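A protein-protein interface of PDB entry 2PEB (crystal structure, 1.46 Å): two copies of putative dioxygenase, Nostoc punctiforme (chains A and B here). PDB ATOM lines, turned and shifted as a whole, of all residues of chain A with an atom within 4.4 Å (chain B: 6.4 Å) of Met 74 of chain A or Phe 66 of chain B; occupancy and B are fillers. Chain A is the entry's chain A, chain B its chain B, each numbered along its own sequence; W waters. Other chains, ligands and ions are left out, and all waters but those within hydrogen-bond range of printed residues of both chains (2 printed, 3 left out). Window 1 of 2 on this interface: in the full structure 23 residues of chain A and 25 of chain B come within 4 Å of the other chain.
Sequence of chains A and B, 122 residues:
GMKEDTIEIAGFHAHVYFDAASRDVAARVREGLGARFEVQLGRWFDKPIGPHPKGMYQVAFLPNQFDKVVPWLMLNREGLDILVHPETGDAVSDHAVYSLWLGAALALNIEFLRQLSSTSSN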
ATOM      1  N   PHE A  66      14.265   1.153  -9.495  1.00  0.00           N
ATOM      2  CA  PHE A  66      14.834   0.341 -10.539  1.00  0.00           C
ATOM      3  C   PHE A  66      13.793   0.105 -11.618  1.00  0.00           C
ATOM      4  O   PHE A  66      14.082   0.337 -12.820  1.00  0.00           O
ATOM      5  CB  PHE A  66      15.429  -0.962  -9.969  1.00  0.00           C
ATOM      6  CG  PHE A  66      16.039  -1.814 -10.976  1.00  0.00           C
ATOM      7  CD1 PHE A  66      17.377  -1.671 -11.325  1.00  0.00           C
ATOM      8  CD2 PHE A  66      15.283  -2.800 -11.611  1.00  0.00           C
ATOM      9  CE1 PHE A  66      17.947  -2.474 -12.271  1.00  0.00           C
ATOM     10  CE2 PHE A  66      15.860  -3.601 -12.565  1.00  0.00           C
ATOM     11  CZ  PHE A  66      17.196  -3.439 -12.917  1.00  0.00           C
ATOM     12  N   ASP A  67      12.561  -0.160 -11.214  1.00  0.00           N
ATOM     13  CA  ASP A  67      11.506  -0.445 -12.213  1.00  0.00           C
ATOM     14  C   ASP A  67      10.845   0.840 -12.757  1.00  0.00           C
ATOM     15  O   ASP A  67       9.888   0.784 -13.568  1.00  0.00           O
ATOM     16  CB  ASP A  67      10.493  -1.458 -11.681  1.00  0.00           C
ATOM     17  CG  ASP A  67       9.607  -0.903 -10.619  1.00  0.00           C
ATOM     18  OD1 ASP A  67       9.669   0.319 -10.318  1.00  0.00           O
ATOM     19  OD2 ASP A  67       8.825  -1.715 -10.099  1.00  0.00           O
ATOM     20  N   VAL A  70      14.874   2.368 -15.067  1.00  0.00           N
ATOM     21  CA  VAL A  70      15.487   1.513 -16.063  1.00  0.00           C
ATOM     22  C   VAL A  70      14.530   1.286 -17.266  1.00  0.00           C
ATOM     23  O   VAL A  70      14.891   1.551 -18.414  1.00  0.00           O
ATOM     24  CB  VAL A  70      16.022   0.209 -15.466  1.00  0.00           C
ATOM     25  CG1 VAL A  70      16.552  -0.710 -16.594  1.00  0.00           C
ATOM     26  CG2 VAL A  70      17.182   0.531 -14.456  1.00  0.00           C
ATOM     27  N   PRO A  71      13.255   0.950 -16.992  1.00  0.00           N
ATOM     28  CA  PRO A  71      12.304   0.936 -18.142  1.00  0.00           C
ATOM     29  C   PRO A  71      12.171   2.266 -18.882  1.00  0.00           C
ATOM     30  O   PRO A  71      12.064   2.277 -20.117  1.00  0.00           O
ATOM     31  CB  PRO A  71      11.013   0.447 -17.517  1.00  0.00           C
ATOM     32  CG  PRO A  71      11.430  -0.306 -16.278  1.00  0.00           C
ATOM     33  CD  PRO A  71      12.600   0.509 -15.751  1.00  0.00           C
ATOM     34  N   TRP A  72      12.245   3.390 -18.160  1.00  0.00           N
ATOM     35  CA  TRP A  72      12.245   4.674 -18.824  1.00  0.00           C
ATOM     36  C   TRP A  72      13.412   4.845 -19.768  1.00  0.00           C
ATOM     37  O   TRP A  72      13.225   5.286 -20.906  1.00  0.00           O
ATOM     38  CB  TRP A  72      12.151   5.830 -17.843  1.00  0.00           C
ATOM     39  CG  TRP A  72      11.868   7.142 -18.473  1.00  0.00           C
ATOM     40  CD1 TRP A  72      10.643   7.681 -18.772  1.00  0.00           C
ATOM     41  CD2 TRP A  72      12.847   8.123 -18.882  1.00  0.00           C
ATOM     42  NE1 TRP A  72      10.810   8.930 -19.337  1.00  0.00           N
ATOM     43  CE2 TRP A  72      12.153   9.223 -19.418  1.00  0.00           C
ATOM     44  CE3 TRP A  72      14.254   8.175 -18.835  1.00  0.00           C
ATOM     45  CZ2 TRP A  72      12.808  10.334 -19.925  1.00  0.00           C
ATOM     46  CZ3 TRP A  72      14.903   9.307 -19.338  1.00  0.00           C
ATOM     47  CH2 TRP A  72      14.178  10.365 -19.864  1.00  0.00           C
ATOM     48  N   LEU A  73      14.625   4.561 -19.323  1.00  0.00           N
ATOM     49  CA  LEU A  73      15.803   4.612 -20.169  1.00  0.00           C
ATOM     50  C   LEU A  73      15.754   3.614 -21.336  1.00  0.00           C
ATOM     51  O   LEU A  73      16.211   3.899 -22.447  1.00  0.00           O
ATOM     52  CB  LEU A  73      17.049   4.394 -19.303  1.00  0.00           C
ATOM     53  CG  LEU A  73      17.420   5.521 -18.328  1.00  0.00           C
ATOM     54  CD1 LEU A  73      18.561   5.047 -17.395  1.00  0.00           C
ATOM     55  CD2 LEU A  73      17.784   6.714 -19.145  1.00  0.00           C
ATOM     56  N   MET A  74      15.145   2.462 -21.092  1.00  0.00           N
ATOM     57  CA  MET A  74      14.939   1.504 -22.174  1.00  0.00           C
ATOM     58  C   MET A  74      14.289   2.128 -23.386  1.00  0.00           C
ATOM     59  O   MET A  74      14.667   1.889 -24.538  1.00  0.00           O
ATOM     60  CB  MET A  74      14.094   0.331 -21.705  1.00  0.00           C
ATOM     61  CG  MET A  74      14.924  -0.776 -20.999  1.00  0.00           C
ATOM     62  SD  MET A  74      14.025  -2.034 -19.875  1.00  0.00           S
ATOM     63  CE  MET A  74      14.271  -3.480 -20.984  1.00  0.00           C
ATOM     64  N   LEU A  75      13.280   2.981 -23.085  1.00  0.00           N
ATOM     65  CA  LEU A  75      12.454   3.553 -24.069  1.00  0.00           C
ATOM     66  C   LEU A  75      12.995   4.900 -24.539  1.00  0.00           C
ATOM     67  O   LEU A  75      12.735   5.312 -25.680  1.00  0.00           O
ATOM     68  CB  LEU A  75      11.031   3.761 -23.553  1.00  0.00           C
ATOM     69  CG  LEU A  75      10.233   2.526 -23.161  1.00  0.00           C
ATOM     70  CD1 LEU A  75       8.783   2.922 -22.743  1.00  0.00           C
ATOM     71  CD2 LEU A  75      10.211   1.564 -24.305  1.00  0.00           C
ATOM     72  N   ASN A  76      13.769   5.595 -23.700  1.00  0.00           N
ATOM     73  CA  ASN A  76      14.045   7.035 -23.924  1.00  0.00           C
ATOM     74  C   ASN A  76      15.531   7.402 -23.993  1.00  0.00           C
ATOM     75  O   ASN A  76      15.888   8.589 -24.083  1.00  0.00           O
ATOM     76  CB  ASN A  76      13.378   7.900 -22.844  1.00  0.00           C
ATOM     77  CG  ASN A  76      11.899   7.881 -22.929  1.00  0.00           C
ATOM     78  OD1 ASN A  76      11.334   8.509 -23.826  1.00  0.00           O
ATOM     79  ND2 ASN A  76      11.249   7.200 -22.004  1.00  0.00           N
ATOM     80  N   LEU A 102      22.362  -1.056 -21.678  1.00  0.00           N
ATOM     81  CA  LEU A 102      21.417  -0.576 -22.671  1.00  0.00           C
ATOM     82  C   LEU A 102      22.253  -0.020 -23.817  1.00  0.00           C
ATOM     83  O   LEU A 102      23.187   0.721 -23.586  1.00  0.00           O
ATOM     84  CB  LEU A 102      20.524   0.502 -22.076  1.00  0.00           C
ATOM     85  CG  LEU A 102      19.979   0.268 -20.664  1.00  0.00           C
ATOM     86  CD1 LEU A 102      19.057   1.428 -20.340  1.00  0.00           C
ATOM     87  CD2 LEU A 102      19.261  -1.063 -20.538  1.00  0.00           C
ATOM     88  N   ILE B   9       4.538  -0.151 -21.558  1.00  0.00           N
ATOM     89  CA  ILE B   9       5.121  -1.471 -21.346  1.00  0.00           C
ATOM     90  C   ILE B   9       4.127  -2.402 -20.648  1.00  0.00           C
ATOM     91  O   ILE B   9       3.774  -2.193 -19.493  1.00  0.00           O
ATOM     92  CB  ILE B   9       6.417  -1.429 -20.538  1.00  0.00           C
ATOM     93  CG1 ILE B   9       7.404  -0.483 -21.222  1.00  0.00           C
ATOM     94  CG2 ILE B   9       6.948  -2.876 -20.369  1.00  0.00           C
ATOM     95  CD1 ILE B   9       8.739  -0.350 -20.495  1.00  0.00           C
ATOM     96  N   PHE B  12       7.377  -7.858 -19.735  1.00  0.00           N
ATOM     97  CA  PHE B  12       8.708  -8.094 -20.251  1.00  0.00           C
ATOM     98  C   PHE B  12       8.918  -9.575 -20.590  1.00  0.00           C
ATOM     99  O   PHE B  12       8.266 -10.443 -20.003  1.00  0.00           O
ATOM    100  CB  PHE B  12       9.782  -7.715 -19.210  1.00  0.00           C
ATOM    101  CG  PHE B  12       9.752  -6.280 -18.818  1.00  0.00           C
ATOM    102  CD1 PHE B  12       8.884  -5.833 -17.833  1.00  0.00           C
ATOM    103  CD2 PHE B  12      10.575  -5.359 -19.481  1.00  0.00           C
ATOM    104  CE1 PHE B  12       8.842  -4.480 -17.482  1.00  0.00           C
ATOM    105  CE2 PHE B  12      10.564  -3.987 -19.132  1.00  0.00           C
ATOM    106  CZ  PHE B  12       9.690  -3.547 -18.166  1.00  0.00           C
ATOM    107  N   PHE B  61       6.963 -11.995 -17.762  1.00  0.00           N
ATOM    108  CA  PHE B  61       6.443 -11.466 -16.520  1.00  0.00           C
ATOM    109  C   PHE B  61       5.812 -10.105 -16.717  1.00  0.00           C
ATOM    110  O   PHE B  61       6.116  -9.363 -17.674  1.00  0.00           O
ATOM    111  CB  PHE B  61       7.521 -11.441 -15.431  1.00  0.00           C
ATOM    112  CG  PHE B  61       8.846 -10.837 -15.861  1.00  0.00           C
ATOM    113  CD1 PHE B  61       9.844 -11.643 -16.430  1.00  0.00           C
ATOM    114  CD2 PHE B  61       9.126  -9.474 -15.675  1.00  0.00           C
ATOM    115  CE1 PHE B  61      11.073 -11.112 -16.807  1.00  0.00           C
ATOM    116  CE2 PHE B  61      10.369  -8.958 -16.055  1.00  0.00           C
ATOM    117  CZ  PHE B  61      11.320  -9.768 -16.624  1.00  0.00           C
ATOM    118  N   LEU B  62       4.903  -9.794 -15.820  1.00  0.00           N
ATOM    119  CA  LEU B  62       4.279  -8.503 -15.783  1.00  0.00           C
ATOM    120  C   LEU B  62       5.249  -7.454 -15.253  1.00  0.00           C
ATOM    121  O   LEU B  62       6.291  -7.781 -14.693  1.00  0.00           O
ATOM    122  CB  LEU B  62       3.020  -8.560 -14.937  1.00  0.00           C
ATOM    123  CG  LEU B  62       1.818  -9.340 -15.475  1.00  0.00           C
ATOM    124  CD1 LEU B  62       0.641  -9.179 -14.529  1.00  0.00           C
ATOM    125  CD2 LEU B  62       1.457  -8.846 -16.873  1.00  0.00           C
ATOM    126  N   PRO B  63       4.956  -6.162 -15.517  1.00  0.00           N
ATOM    127  CA  PRO B  63       5.914  -5.116 -15.098  1.00  0.00           C
ATOM    128  C   PRO B  63       6.269  -5.118 -13.610  1.00  0.00           C
ATOM    129  O   PRO B  63       7.401  -4.783 -13.277  1.00  0.00           O
ATOM    130  CB  PRO B  63       5.225  -3.819 -15.517  1.00  0.00           C
ATOM    131  CG  PRO B  63       4.284  -4.239 -16.637  1.00  0.00           C
ATOM    132  CD  PRO B  63       3.821  -5.608 -16.258  1.00  0.00           C
ATOM    133  N   ASN B  64       5.348  -5.539 -12.744  1.00  0.00           N
ATOM    134  CA  ASN B  64       5.590  -5.599 -11.277  1.00  0.00           C
ATOM    135  C   ASN B  64       6.640  -6.627 -10.820  1.00  0.00           C
ATOM    136  O   ASN B  64       6.978  -6.672  -9.644  1.00  0.00           O
ATOM    137  CB  ASN B  64       4.302  -5.705 -10.446  1.00  0.00           C
ATOM    138  CG  ASN B  64       3.597  -7.037 -10.599  1.00  0.00           C
ATOM    139  OD1 ASN B  64       4.180  -8.028 -10.997  1.00  0.00           O
ATOM    140  ND2 ASN B  64       2.313  -7.051 -10.293  1.00  0.00           N
ATOM    141  N   GLN B  65       7.098  -7.488 -11.715  1.00  0.00           N
ATOM    142  CA  GLN B  65       8.233  -8.380 -11.424  1.00  0.00           C
ATOM    143  C   GLN B  65       9.574  -7.897 -11.959  1.00  0.00           C
ATOM    144  O   GLN B  65      10.598  -8.537 -11.763  1.00  0.00           O
ATOM    145  CB  GLN B  65       7.965  -9.793 -11.963  1.00  0.00           C
ATOM    146  CG  GLN B  65       6.689 -10.403 -11.465  1.00  0.00           C
ATOM    147  CD  GLN B  65       6.777 -10.730 -10.029  1.00  0.00           C
ATOM    148  OE1 GLN B  65       7.601 -11.565  -9.619  1.00  0.00           O
ATOM    149  NE2 GLN B  65       5.972 -10.061  -9.227  1.00  0.00           N
ATOM    150  N   PHE B  66       9.604  -6.787 -12.685  1.00  0.00           N
ATOM    151  CA  PHE B  66      10.836  -6.345 -13.322  1.00  0.00           C
ATOM    152  C   PHE B  66      11.956  -6.143 -12.288  1.00  0.00           C
ATOM    153  O   PHE B  66      13.114  -6.585 -12.529  1.00  0.00           O
ATOM    154  CB  PHE B  66      10.565  -5.072 -14.106  1.00  0.00           C
ATOM    155  CG  PHE B  66      11.755  -4.557 -14.860  1.00  0.00           C
ATOM    156  CD1 PHE B  66      12.106  -5.066 -16.136  1.00  0.00           C
ATOM    157  CD2 PHE B  66      12.553  -3.565 -14.319  1.00  0.00           C
ATOM    158  CE1 PHE B  66      13.195  -4.591 -16.863  1.00  0.00           C
ATOM    159  CE2 PHE B  66      13.653  -3.104 -15.033  1.00  0.00           C
ATOM    160  CZ  PHE B  66      13.935  -3.583 -16.327  1.00  0.00           C
ATOM    161  N   ASP B  67      11.632  -5.503 -11.163  1.00  0.00           N
ATOM    162  CA  ASP B  67      12.640  -5.225 -10.111  1.00  0.00           C
ATOM    163  C   ASP B  67      12.886  -6.391  -9.173  1.00  0.00           C
ATOM    164  O   ASP B  67      13.693  -6.274  -8.229  1.00  0.00           O
ATOM    165  CB  ASP B  67      12.297  -3.953  -9.308  1.00  0.00           C
ATOM    166  CG  ASP B  67      11.119  -4.123  -8.374  1.00  0.00           C
ATOM    167  OD1 ASP B  67      10.619  -5.250  -8.152  1.00  0.00           O
ATOM    168  OD2 ASP B  67      10.679  -3.068  -7.835  1.00  0.00           O
ATOM    169  N   LYS B  68      12.245  -7.528  -9.454  1.00  0.00           N
ATOM    170  CA  LYS B  68      12.460  -8.794  -8.738  1.00  0.00           C
ATOM    171  C   LYS B  68      13.331  -9.735  -9.597  1.00  0.00           C
ATOM    172  O   LYS B  68      14.435 -10.134  -9.231  1.00  0.00           O
ATOM    173  CB  LYS B  68      11.108  -9.415  -8.402  1.00  0.00           C
ATOM    174  CG  LYS B  68      10.240  -8.478  -7.538  1.00  0.00           C
ATOM    175  CD  LYS B  68       8.945  -9.129  -7.095  1.00  0.00           C
ATOM    176  CE  LYS B  68       8.218  -8.280  -6.044  1.00  0.00           C
ATOM    177  NZ  LYS B  68       6.985  -8.963  -5.549  1.00  0.00           N
ATOM    178  N   VAL B  69      12.829 -10.025 -10.790  1.00  0.00           N
ATOM    179  CA  VAL B  69      13.507 -10.912 -11.717  1.00  0.00           C
ATOM    180  C   VAL B  69      14.835 -10.372 -12.226  1.00  0.00           C
ATOM    181  O   VAL B  69      15.844 -11.049 -12.270  1.00  0.00           O
ATOM    182  CB  VAL B  69      12.573 -11.242 -12.937  1.00  0.00           C
ATOM    183  CG1 VAL B  69      13.352 -12.040 -13.993  1.00  0.00           C
ATOM    184  CG2 VAL B  69      11.339 -12.046 -12.515  1.00  0.00           C
ATOM    185  N   VAL B  70      14.845  -9.131 -12.687  1.00  0.00           N
ATOM    186  CA  VAL B  70      16.031  -8.635 -13.357  1.00  0.00           C
ATOM    187  C   VAL B  70      17.207  -8.493 -12.414  1.00  0.00           C
ATOM    188  O   VAL B  70      18.282  -8.965 -12.747  1.00  0.00           O
ATOM    189  CB  VAL B  70      15.765  -7.370 -14.265  1.00  0.00           C
ATOM    190  CG1 VAL B  70      17.052  -6.866 -14.874  1.00  0.00           C
ATOM    191  CG2 VAL B  70      14.666  -7.714 -15.385  1.00  0.00           C
ATOM    192  N   PRO B  71      17.022  -7.826 -11.261  1.00  0.00           N
ATOM    193  CA  PRO B  71      18.114  -7.842 -10.231  1.00  0.00           C
ATOM    194  C   PRO B  71      18.584  -9.232  -9.772  1.00  0.00           C
ATOM    195  O   PRO B  71      19.767  -9.425  -9.581  1.00  0.00           O
ATOM    196  CB  PRO B  71      17.480  -7.039  -9.073  1.00  0.00           C
ATOM    197  CG  PRO B  71      16.590  -6.093  -9.787  1.00  0.00           C
ATOM    198  CD  PRO B  71      15.936  -6.974 -10.789  1.00  0.00           C
ATOM    199  N   VAL B  84      16.666  -8.980 -22.222  1.00  0.00           N
ATOM    200  CA  VAL B  84      15.390  -8.626 -21.597  1.00  0.00           C
ATOM    201  C   VAL B  84      14.781  -7.528 -22.434  1.00  0.00           C
ATOM    202  O   VAL B  84      15.417  -6.545 -22.729  1.00  0.00           O
ATOM    203  CB  VAL B  84      15.548  -8.147 -20.118  1.00  0.00           C
ATOM    204  CG1 VAL B  84      14.179  -7.710 -19.541  1.00  0.00           C
ATOM    205  CG2 VAL B  84      16.214  -9.217 -19.245  1.00  0.00           C
ATOM    206  N   HIS B  85      13.520  -7.693 -22.819  1.00  0.00           N
ATOM    207  CA  HIS B  85      12.873  -6.680 -23.638  1.00  0.00           C
ATOM    208  C   HIS B  85      11.463  -6.426 -23.171  1.00  0.00           C
ATOM    209  O   HIS B  85      10.818  -7.324 -22.647  1.00  0.00           O
ATOM    210  CB  HIS B  85      12.921  -7.044 -25.136  1.00  0.00           C
ATOM    211  CG  HIS B  85      12.120  -8.248 -25.537  1.00  0.00           C
ATOM    212  ND1 HIS B  85      10.750  -8.216 -25.707  1.00  0.00           N
ATOM    213  CD2 HIS B  85      12.502  -9.504 -25.874  1.00  0.00           C
ATOM    214  CE1 HIS B  85      10.321  -9.410 -26.079  1.00  0.00           C
ATOM    215  NE2 HIS B  85      11.365 -10.205 -26.204  1.00  0.00           N
ATOM    216  N   PRO B  86      11.007  -5.194 -23.324  1.00  0.00           N
ATOM    217  CA  PRO B  86       9.628  -4.905 -23.016  1.00  0.00           C
ATOM    218  C   PRO B  86       8.703  -5.451 -24.097  1.00  0.00           C
ATOM    219  O   PRO B  86       9.139  -5.896 -25.142  1.00  0.00           O
ATOM    220  CB  PRO B  86       9.627  -3.373 -22.980  1.00  0.00           C
ATOM    221  CG  PRO B  86      10.576  -2.992 -23.961  1.00  0.00           C
ATOM    222  CD  PRO B  86      11.682  -3.998 -23.868  1.00  0.00           C
ATOM    223  N   VAL B  97      15.830  -2.074 -29.991  1.00  0.00           N
ATOM    224  CA  VAL B  97      16.030  -0.701 -29.493  1.00  0.00           C
ATOM    225  C   VAL B  97      15.745  -0.647 -27.985  1.00  0.00           C
ATOM    226  O   VAL B  97      16.537  -0.051 -27.241  1.00  0.00           O
ATOM    227  CB  VAL B  97      15.133   0.340 -30.257  1.00  0.00           C
ATOM    228  CG1 VAL B  97      15.454   1.764 -29.787  1.00  0.00           C
ATOM    229  CG2 VAL B  97      15.233   0.192 -31.772  1.00  0.00           C
ATOM    230  N   TYR B  98      14.621  -1.216 -27.543  1.00  0.00           N
ATOM    231  CA  TYR B  98      14.155  -1.080 -26.162  1.00  0.00           C
ATOM    232  C   TYR B  98      14.623  -2.095 -25.173  1.00  0.00           C
ATOM    233  O   TYR B  98      14.137  -2.125 -24.051  1.00  0.00           O
ATOM    234  CB  TYR B  98      12.650  -1.088 -26.137  1.00  0.00           C
ATOM    235  CG  TYR B  98      11.969  -0.066 -26.964  1.00  0.00           C
ATOM    236  CD1 TYR B  98      12.566   1.150 -27.299  1.00  0.00           C
ATOM    237  CD2 TYR B  98      10.669  -0.288 -27.360  1.00  0.00           C
ATOM    238  CE1 TYR B  98      11.887   2.083 -28.044  1.00  0.00           C
ATOM    239  CE2 TYR B  98       9.979   0.621 -28.059  1.00  0.00           C
ATOM    240  CZ  TYR B  98      10.586   1.819 -28.435  1.00  0.00           C
ATOM    241  OH  TYR B  98       9.880   2.721 -29.166  1.00  0.00           O
ATOM    242  N   SER B  99      15.581  -2.923 -25.593  1.00  0.00           N
ATOM    243  CA  SER B  99      16.007  -4.027 -24.784  1.00  0.00           C
ATOM    244  C   SER B  99      17.267  -3.712 -23.976  1.00  0.00           C
ATOM    245  O   SER B  99      17.877  -2.648 -24.117  1.00  0.00           O
ATOM    246  CB  SER B  99      16.247  -5.223 -25.680  1.00  0.00           C
ATOM    247  OG  SER B  99      17.142  -4.873 -26.724  1.00  0.00           O
ATOM    248  N   LEU B 100      17.572  -4.613 -23.066  1.00  0.00           N
ATOM    249  CA  LEU B 100      18.852  -4.601 -22.398  1.00  0.00           C
ATOM    250  C   LEU B 100      19.455  -5.989 -22.420  1.00  0.00           C
ATOM    251  O   LEU B 100      18.757  -6.980 -22.618  1.00  0.00           O
ATOM    252  CB  LEU B 100      18.612  -4.177 -20.942  1.00  0.00           C
ATOM    253  CG  LEU B 100      17.829  -5.090 -19.982  1.00  0.00           C
ATOM    254  CD1 LEU B 100      18.640  -6.193 -19.448  1.00  0.00           C
ATOM    255  CD2 LEU B 100      17.196  -4.293 -18.797  1.00  0.00           C
HETATM  256  O   HOH W   1       8.209  -2.094 -14.318  1.00  0.00           O
HETATM  257  O   HOH W   2      11.982  -0.790  -8.463  1.00  0.00           O
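OD2 of Asp 67 of chain A sits close to OD2 of Asp 67 of chain B (3.2 Å).
O of Val 84 of chain B is in hydrogen-bond range of N of Leu 100 of chain B (2.9 Å).
Phe 66 of chain B touches Phe 66 of chain A (CE2 to CE2, 3.3 Å).
CZ of Phe 66 of chain A touches CG1 of Val 70 of chain B, 3.9 Å away.
CE2 of Phe 66 of chain A touches CG of Pro 71 of chain B (3.8 Å).
CG1 of Val 70 of chain A touches CZ of Phe 66 of chain B, 3.9 Å away.
Ile 9 of chain B touches Pro 71 of chain A.
CE of Met 74 of chain A touches O of Val 84 of chain B, 3.7 Å away.
Tyr 98 of chain B touches Met 74 of chain A (O to CE, 3.4 Å).
CD1 of Leu 75 of chain A touches CD1 of Ile 9 of chain B, 3.97 Å away.
Tyr 98 of chain B touches Leu 75 of chain A (CG to CD2, 3.6 Å).
Leu 102 of chain A touches Leu 100 of chain B.
Of the printed residues of chain B, Val 70 of chain A touches Phe 66 (3.9 Å).
Of the printed residues of chain B, Pro 71 of chain A touches Ile 9 (3.8 Å) and Phe 66 (3.8 Å).
Of chain B, only Phe 66 (3.9 Å), Val 84 (3.7 Å), Pro 86 (3.9 Å), Val 97 (3.8 Å), Tyr 98 (3.4 Å) and Leu 100 (3.7 Å) come within 4 Å of Met 74 of chain A.
Phe 12 of chain B touches none of the printed residues of chain A.
Of chain A, only Phe 66, Asp 67, Val 70, Pro 71 and Met 74 come within 4 Å of Phe 66 of chain B.
The nearest residue of chain B that does not touch Met 74 of chain A is Phe 12 of chain B (4.04 Å).
Hydrophobic or aromatic side chains of chain A that line the printed part of chain B: Phe 66, Val 70, Pro 71, Met 74, Leu 75 and Leu 102.
Hydrophobic or aromatic side chains of chain B within 4 Å of the printed part of chain A: Ile 9, Phe 66, Val 70, Pro 71, Pro 86, Tyr 98 and Leu 100.
Among the printed residues, 18 pairs touch across the chains.
Phe 66 of chain A touches its own counterpart, Phe 66 of chain B.
Phe 66 of chain A touches Asp 67 of chain B, and with the chains exchanged Asp 67 of chain A touches Phe 66 of chain B.
Phe 66 of chain A touches Pro 71 of chain B, and with the chains exchanged Pro 71 of chain A touches Phe 66 of chain B.
Asp 67 of chain A touches its own counterpart, Asp 67 of chain B.
Water W2 lies within hydrogen-bond range of the side-chain carboxylate of Asp 67 of chain B (2.7 Å), the backbone NH of Asp 67 of chain A (2.9 Å) and the backbone NH of Phe 66 of chain A (3.2 Å).
Water W1 bridges O of Pro 63 of chain B and O of Asp 67 of chain A.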
